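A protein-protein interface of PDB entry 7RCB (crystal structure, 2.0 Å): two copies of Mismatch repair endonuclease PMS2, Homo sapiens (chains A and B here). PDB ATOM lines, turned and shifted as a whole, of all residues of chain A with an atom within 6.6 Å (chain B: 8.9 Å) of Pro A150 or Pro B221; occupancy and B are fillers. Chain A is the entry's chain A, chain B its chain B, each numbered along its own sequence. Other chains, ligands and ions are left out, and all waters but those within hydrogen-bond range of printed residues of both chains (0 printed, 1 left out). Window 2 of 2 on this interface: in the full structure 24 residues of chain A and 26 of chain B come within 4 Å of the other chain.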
ATOM      1  N   CYS A 125      -7.694  20.656 -12.480  1.00  0.00           N
ATOM      2  CA  CYS A 125      -7.786  21.782 -11.560  1.00  0.00           C
ATOM      3  C   CYS A 125      -6.739  22.816 -11.944  1.00  0.00           C
ATOM      4  O   CYS A 125      -5.541  22.522 -11.945  1.00  0.00           O
ATOM      5  CB  CYS A 125      -7.602  21.345 -10.107  1.00  0.00           C
ATOM      6  SG  CYS A 125      -7.880  22.694  -8.946  1.00  0.00           S
ATOM      7  N   VAL A 131     -11.873  24.683  -6.673  1.00  0.00           N
ATOM      8  CA  VAL A 131     -11.990  23.233  -6.666  1.00  0.00           C
ATOM      9  C   VAL A 131     -11.815  22.735  -8.097  1.00  0.00           C
ATOM     10  O   VAL A 131     -12.029  23.468  -9.066  1.00  0.00           O
ATOM     11  CB  VAL A 131     -13.345  22.761  -6.086  1.00  0.00           C
ATOM     12  CG1 VAL A 131     -14.488  23.148  -7.013  1.00  0.00           C
ATOM     13  CG2 VAL A 131     -13.348  21.260  -5.827  1.00  0.00           C
ATOM     14  N   GLY A 132     -11.388  21.481  -8.224  1.00  0.00           N
ATOM     15  CA  GLY A 132     -11.273  20.857  -9.521  1.00  0.00           C
ATOM     16  C   GLY A 132     -12.619  20.436 -10.082  1.00  0.00           C
ATOM     17  O   GLY A 132     -13.671  20.592  -9.465  1.00  0.00           O
ATOM     18  N   THR A 133     -12.570  19.875 -11.288  1.00  0.00           N
ATOM     19  CA  THR A 133     -13.754  19.432 -12.007  1.00  0.00           C
ATOM     20  C   THR A 133     -13.463  18.104 -12.689  1.00  0.00           C
ATOM     21  O   THR A 133     -12.341  17.866 -13.142  1.00  0.00           O
ATOM     22  CB  THR A 133     -14.192  20.471 -13.052  1.00  0.00           C
ATOM     23  OG1 THR A 133     -14.430  21.727 -12.408  1.00  0.00           O
ATOM     24  CG2 THR A 133     -15.455  20.034 -13.755  1.00  0.00           C
ATOM     25  N   PRO A 148     -18.000  19.172  -9.571  1.00  0.00           N
ATOM     26  CA  PRO A 148     -16.835  19.545  -8.764  1.00  0.00           C
ATOM     27  C   PRO A 148     -16.099  18.313  -8.264  1.00  0.00           C
ATOM     28  O   PRO A 148     -16.705  17.300  -7.910  1.00  0.00           O
ATOM     29  CB  PRO A 148     -17.444  20.348  -7.609  1.00  0.00           C
ATOM     30  CG  PRO A 148     -18.740  20.854  -8.145  1.00  0.00           C
ATOM     31  CD  PRO A 148     -19.241  19.780  -9.063  1.00  0.00           C
ATOM     32  N   TYR A 149     -14.781  18.418  -8.228  1.00  0.00           N
ATOM     33  CA  TYR A 149     -13.917  17.271  -7.958  1.00  0.00           C
ATOM     34  C   TYR A 149     -12.658  17.791  -7.288  1.00  0.00           C
ATOM     35  O   TYR A 149     -11.747  18.292  -7.963  1.00  0.00           O
ATOM     36  CB  TYR A 149     -13.596  16.541  -9.258  1.00  0.00           C
ATOM     37  CG  TYR A 149     -12.874  15.227  -9.116  1.00  0.00           C
ATOM     38  CD1 TYR A 149     -13.556  14.079  -8.738  1.00  0.00           C
ATOM     39  CD2 TYR A 149     -11.521  15.124  -9.410  1.00  0.00           C
ATOM     40  CE1 TYR A 149     -12.905  12.869  -8.627  1.00  0.00           C
ATOM     41  CE2 TYR A 149     -10.862  13.916  -9.304  1.00  0.00           C
ATOM     42  CZ  TYR A 149     -11.560  12.790  -8.912  1.00  0.00           C
ATOM     43  OH  TYR A 149     -10.911  11.580  -8.800  1.00  0.00           O
ATOM     44  N   PRO A 150     -12.552  17.674  -5.964  1.00  0.00           N
ATOM     45  CA  PRO A 150     -11.353  18.176  -5.275  1.00  0.00           C
ATOM     46  C   PRO A 150     -10.148  17.322  -5.634  1.00  0.00           C
ATOM     47  O   PRO A 150     -10.129  16.115  -5.389  1.00  0.00           O
ATOM     48  CB  PRO A 150     -11.719  18.061  -3.789  1.00  0.00           C
ATOM     49  CG  PRO A 150     -13.203  17.950  -3.764  1.00  0.00           C
ATOM     50  CD  PRO A 150     -13.579  17.222  -5.014  1.00  0.00           C
ATOM     51  N   ARG A 151      -9.136  17.960  -6.209  1.00  0.00           N
ATOM     52  CA  ARG A 151      -7.935  17.286  -6.676  1.00  0.00           C
ATOM     53  C   ARG A 151      -6.831  18.323  -6.771  1.00  0.00           C
ATOM     54  O   ARG A 151      -7.116  19.522  -6.856  1.00  0.00           O
ATOM     55  CB  ARG A 151      -8.168  16.611  -8.039  1.00  0.00           C
ATOM     56  CG  ARG A 151      -8.698  17.546  -9.121  1.00  0.00           C
ATOM     57  CD  ARG A 151      -8.216  17.108 -10.486  1.00  0.00           C
ATOM     58  NE  ARG A 151      -6.768  17.236 -10.572  1.00  0.00           N
ATOM     59  CZ  ARG A 151      -5.974  16.399 -11.222  1.00  0.00           C
ATOM     60  NH1 ARG A 151      -6.455  15.352 -11.872  1.00  0.00           N
ATOM     61  NH2 ARG A 151      -4.661  16.603 -11.197  1.00  0.00           N
ATOM     62  N   PRO A 152      -5.568  17.902  -6.743  1.00  0.00           N
ATOM     63  CA  PRO A 152      -4.476  18.868  -6.891  1.00  0.00           C
ATOM     64  C   PRO A 152      -4.427  19.452  -8.295  1.00  0.00           C
ATOM     65  O   PRO A 152      -5.024  18.933  -9.241  1.00  0.00           O
ATOM     66  CB  PRO A 152      -3.221  18.042  -6.586  1.00  0.00           C
ATOM     67  CG  PRO A 152      -3.617  16.639  -6.850  1.00  0.00           C
ATOM     68  CD  PRO A 152      -5.064  16.544  -6.474  1.00  0.00           C
ATOM     69  N   ILE B 193      -3.086   5.658   1.238  1.00  0.00           N
ATOM     70  CA  ILE B 193      -4.524   5.447   1.366  1.00  0.00           C
ATOM     71  C   ILE B 193      -5.205   6.673   1.967  1.00  0.00           C
ATOM     72  O   ILE B 193      -6.247   7.125   1.477  1.00  0.00           O
ATOM     73  CB  ILE B 193      -4.789   4.180   2.196  1.00  0.00           C
ATOM     74  CG1 ILE B 193      -4.384   2.939   1.397  1.00  0.00           C
ATOM     75  CG2 ILE B 193      -6.249   4.103   2.612  1.00  0.00           C
ATOM     76  CD1 ILE B 193      -4.248   1.688   2.238  1.00  0.00           C
ATOM     77  N   ILE B 194      -4.633   7.231   3.037  1.00  0.00           N
ATOM     78  CA  ILE B 194      -5.332   8.273   3.786  1.00  0.00           C
ATOM     79  C   ILE B 194      -5.144   9.664   3.192  1.00  0.00           C
ATOM     80  O   ILE B 194      -5.945  10.567   3.476  1.00  0.00           O
ATOM     81  CB  ILE B 194      -4.887   8.261   5.257  1.00  0.00           C
ATOM     82  CG1 ILE B 194      -5.951   8.912   6.142  1.00  0.00           C
ATOM     83  CG2 ILE B 194      -3.542   8.952   5.425  1.00  0.00           C
ATOM     84  CD1 ILE B 194      -7.250   8.146   6.187  1.00  0.00           C
ATOM     85  N   SER B 195      -4.124   9.864   2.360  1.00  0.00           N
ATOM     86  CA  SER B 195      -3.791  11.199   1.864  1.00  0.00           C
ATOM     87  C   SER B 195      -4.587  11.511   0.597  1.00  0.00           C
ATOM     88  O   SER B 195      -4.064  11.553  -0.519  1.00  0.00           O
ATOM     89  CB  SER B 195      -2.292  11.315   1.626  1.00  0.00           C
ATOM     90  OG  SER B 195      -1.569  11.045   2.813  1.00  0.00           O
ATOM     91  N   ALA B 196      -5.884  11.733   0.792  1.00  0.00           N
ATOM     92  CA  ALA B 196      -6.733  12.186  -0.301  1.00  0.00           C
ATOM     93  C   ALA B 196      -6.280  13.559  -0.786  1.00  0.00           C
ATOM     94  O   ALA B 196      -5.869  14.413   0.006  1.00  0.00           O
ATOM     95  CB  ALA B 196      -8.195  12.236   0.149  1.00  0.00           C
ATOM     96  N   GLY B 197      -6.339  13.768  -2.100  1.00  0.00           N
ATOM     97  CA  GLY B 197      -5.926  15.029  -2.680  1.00  0.00           C
ATOM     98  C   GLY B 197      -4.435  15.200  -2.864  1.00  0.00           C
ATOM     99  O   GLY B 197      -4.002  16.271  -3.310  1.00  0.00           O
ATOM    100  N   ILE B 198      -3.637  14.190  -2.529  1.00  0.00           N
ATOM    101  CA  ILE B 198      -2.184  14.269  -2.593  1.00  0.00           C
ATOM    102  C   ILE B 198      -1.671  13.111  -3.429  1.00  0.00           C
ATOM    103  O   ILE B 198      -2.047  11.957  -3.198  1.00  0.00           O
ATOM    104  CB  ILE B 198      -1.550  14.247  -1.191  1.00  0.00           C
ATOM    105  CG1 ILE B 198      -2.041  15.450  -0.384  1.00  0.00           C
ATOM    106  CG2 ILE B 198      -0.032  14.217  -1.291  1.00  0.00           C
ATOM    107  CD1 ILE B 198      -1.746  15.377   1.091  1.00  0.00           C
ATOM    108  N   THR B 217      -0.378   7.250  -6.449  1.00  0.00           N
ATOM    109  CA  THR B 217      -1.769   7.659  -6.374  1.00  0.00           C
ATOM    110  C   THR B 217      -1.989   8.845  -7.300  1.00  0.00           C
ATOM    111  O   THR B 217      -1.047   9.522  -7.712  1.00  0.00           O
ATOM    112  CB  THR B 217      -2.161   8.031  -4.944  1.00  0.00           C
ATOM    113  OG1 THR B 217      -1.334   9.109  -4.484  1.00  0.00           O
ATOM    114  CG2 THR B 217      -1.992   6.837  -4.019  1.00  0.00           C
ATOM    115  N   GLY B 218      -3.249   9.076  -7.647  1.00  0.00           N
ATOM    116  CA  GLY B 218      -3.599  10.088  -8.620  1.00  0.00           C
ATOM    117  C   GLY B 218      -4.105  11.390  -8.042  1.00  0.00           C
ATOM    118  O   GLY B 218      -4.590  12.235  -8.803  1.00  0.00           O
ATOM    119  N   GLY B 219      -3.985  11.596  -6.734  1.00  0.00           N
ATOM    120  CA  GLY B 219      -4.533  12.790  -6.123  1.00  0.00           C
ATOM    121  C   GLY B 219      -6.039  12.759  -6.002  1.00  0.00           C
ATOM    122  O   GLY B 219      -6.683  13.802  -6.115  1.00  0.00           O
ATOM    123  N   SER B 220      -6.616  11.583  -5.769  1.00  0.00           N
ATOM    124  CA  SER B 220      -8.060  11.434  -5.766  1.00  0.00           C
ATOM    125  C   SER B 220      -8.646  11.866  -4.425  1.00  0.00           C
ATOM    126  O   SER B 220      -7.996  11.737  -3.384  1.00  0.00           O
ATOM    127  CB  SER B 220      -8.440   9.984  -6.048  1.00  0.00           C
ATOM    128  OG  SER B 220      -9.845   9.814  -6.065  1.00  0.00           O
ATOM    129  N   PRO B 221      -9.877  12.386  -4.423  1.00  0.00           N
ATOM    130  CA  PRO B 221     -10.481  12.845  -3.165  1.00  0.00           C
ATOM    131  C   PRO B 221     -11.062  11.737  -2.300  1.00  0.00           C
ATOM    132  O   PRO B 221     -11.476  12.025  -1.168  1.00  0.00           O
ATOM    133  CB  PRO B 221     -11.582  13.806  -3.638  1.00  0.00           C
ATOM    134  CG  PRO B 221     -11.941  13.324  -4.996  1.00  0.00           C
ATOM    135  CD  PRO B 221     -10.676  12.776  -5.598  1.00  0.00           C
ATOM    136  N   SER B 222     -11.098  10.490  -2.765  1.00  0.00           N
ATOM    137  CA  SER B 222     -11.719   9.421  -1.997  1.00  0.00           C
ATOM    138  C   SER B 222     -10.682   8.382  -1.603  1.00  0.00           C
ATOM    139  O   SER B 222      -9.807   8.019  -2.396  1.00  0.00           O
ATOM    140  CB  SER B 222     -12.851   8.741  -2.784  1.00  0.00           C
ATOM    141  OG  SER B 222     -12.349   7.894  -3.799  1.00  0.00           O
ATOM    142  N   ILE B 223     -10.804   7.902  -0.365  1.00  0.00           N
ATOM    143  CA  ILE B 223      -9.975   6.804   0.111  1.00  0.00           C
ATOM    144  C   ILE B 223     -10.181   5.566  -0.748  1.00  0.00           C
ATOM    145  O   ILE B 223      -9.241   4.797  -0.980  1.00  0.00           O
ATOM    146  CB  ILE B 223     -10.280   6.549   1.601  1.00  0.00           C
ATOM    147  CG1 ILE B 223      -9.734   7.708   2.442  1.00  0.00           C
ATOM    148  CG2 ILE B 223      -9.716   5.219   2.068  1.00  0.00           C
ATOM    149  CD1 ILE B 223     -10.196   7.694   3.878  1.00  0.00           C
ATOM    150  N   LYS B 224     -11.401   5.365  -1.252  1.00  0.00           N
ATOM    151  CA  LYS B 224     -11.693   4.177  -2.045  1.00  0.00           C
ATOM    152  C   LYS B 224     -10.872   4.152  -3.329  1.00  0.00           C
ATOM    153  O   LYS B 224     -10.309   3.116  -3.701  1.00  0.00           O
ATOM    154  CB  LYS B 224     -13.188   4.115  -2.355  1.00  0.00           C
ATOM    155  CG  LYS B 224     -13.602   2.844  -3.063  1.00  0.00           C
ATOM    156  CD  LYS B 224     -15.100   2.782  -3.257  1.00  0.00           C
ATOM    157  CE  LYS B 224     -15.494   1.460  -3.875  1.00  0.00           C
ATOM    158  NZ  LYS B 224     -16.965   1.241  -3.835  1.00  0.00           N
ATOM    159  N   GLU B 225     -10.796   5.284  -4.029  1.00  0.00           N
ATOM    160  CA  GLU B 225      -9.973   5.328  -5.231  1.00  0.00           C
ATOM    161  C   GLU B 225      -8.491   5.230  -4.893  1.00  0.00           C
ATOM    162  O   GLU B 225      -7.717   4.651  -5.666  1.00  0.00           O
ATOM    163  CB  GLU B 225     -10.287   6.592  -6.033  1.00  0.00           C
ATOM    164  CG  GLU B 225     -11.671   6.539  -6.680  1.00  0.00           C
ATOM    165  CD  GLU B 225     -12.103   7.854  -7.302  1.00  0.00           C
ATOM    166  OE1 GLU B 225     -11.295   8.465  -8.034  1.00  0.00           O
ATOM    167  OE2 GLU B 225     -13.261   8.268  -7.074  1.00  0.00           O
ATOM    168  N   ASN B 226      -8.074   5.785  -3.750  1.00  0.00           N
ATOM    169  CA  ASN B 226      -6.692   5.610  -3.317  1.00  0.00           C
ATOM    170  C   ASN B 226      -6.393   4.144  -3.033  1.00  0.00           C
ATOM    171  O   ASN B 226      -5.301   3.658  -3.341  1.00  0.00           O
ATOM    172  CB  ASN B 226      -6.399   6.469  -2.087  1.00  0.00           C
ATOM    173  CG  ASN B 226      -6.175   7.929  -2.430  1.00  0.00           C
ATOM    174  OD1 ASN B 226      -5.914   8.279  -3.581  1.00  0.00           O
ATOM    175  ND2 ASN B 226      -6.251   8.787  -1.424  1.00  0.00           N
ATOM    176  N   ARG B 294      -6.815  10.545  10.986  1.00  0.00           N
ATOM    177  CA  ARG B 294      -6.064  10.439   9.734  1.00  0.00           C
ATOM    178  C   ARG B 294      -4.594  10.078   9.923  1.00  0.00           C
ATOM    179  O   ARG B 294      -3.847  10.052   8.938  1.00  0.00           O
ATOM    180  CB  ARG B 294      -6.146  11.720   8.892  1.00  0.00           C
ATOM    181  CG  ARG B 294      -7.485  12.459   8.932  1.00  0.00           C
ATOM    182  CD  ARG B 294      -8.545  11.809   8.070  1.00  0.00           C
ATOM    183  NE  ARG B 294      -8.167  11.780   6.663  1.00  0.00           N
ATOM    184  CZ  ARG B 294      -9.006  11.507   5.675  1.00  0.00           C
ATOM    185  NH1 ARG B 294     -10.295  11.311   5.901  1.00  0.00           N
ATOM    186  NH2 ARG B 294      -8.539  11.420   4.432  1.00  0.00           N
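No position is printed for both chains.
Of the 7 pairs that touch across the chains among the printed residues, none has its exchanged pair printed and touching as well.
OH of Tyr A149 lies within hydrogen-bond range of OG of Ser B220 (3.4 Å).
The side-chain carboxylate (OE1) of Glu B225 sits at hydrogen-bond distance from the side-chain hydroxyl (OH) of Tyr A149 (3.2 Å).
Hydrophobic or aromatic side chains of chain A within 4 Å of the printed part of chain B: Tyr A149 and Pro A152.
Among the printed residues, merely in contact across the chains: Pro A152 with Gly B219, Pro A150 with Pro B221, Pro A152 with Gly B197, Tyr A149 with Pro B221 and Arg A151 with Gly B219.
Of chain B, only Ser B220, Pro B221 and Glu B225 come within 4 Å of Tyr A149.
Pro A150 touches just one residue of chain B: Pro B221.
Of the printed residues of chain B, Arg A151 touches Gly B219.
Ser B195 touches none of the printed residues of chain A.
Ile B198 touches none of the printed residues of chain A.
Pro B221 touches two residues of chain A.
Of the printed residues of chain A, Glu B225 touches Tyr A149.
O of Gly A132 sits at hydrogen-bond distance from N of Tyr A149 (2.7 Å).
The backbone carbonyl oxygen (O) of Ser B220 is in hydrogen-bond range of the backbone NH (N) of Gly B197 (2.9 Å).
The side-chain carboxylate of Glu B225 lies within hydrogen-bond range of the side-chain hydroxyl of Ser B220 (2.8 Å).
OG of Ser B222 sits at hydrogen-bond distance from N of Glu B225, at 3.0 Å.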
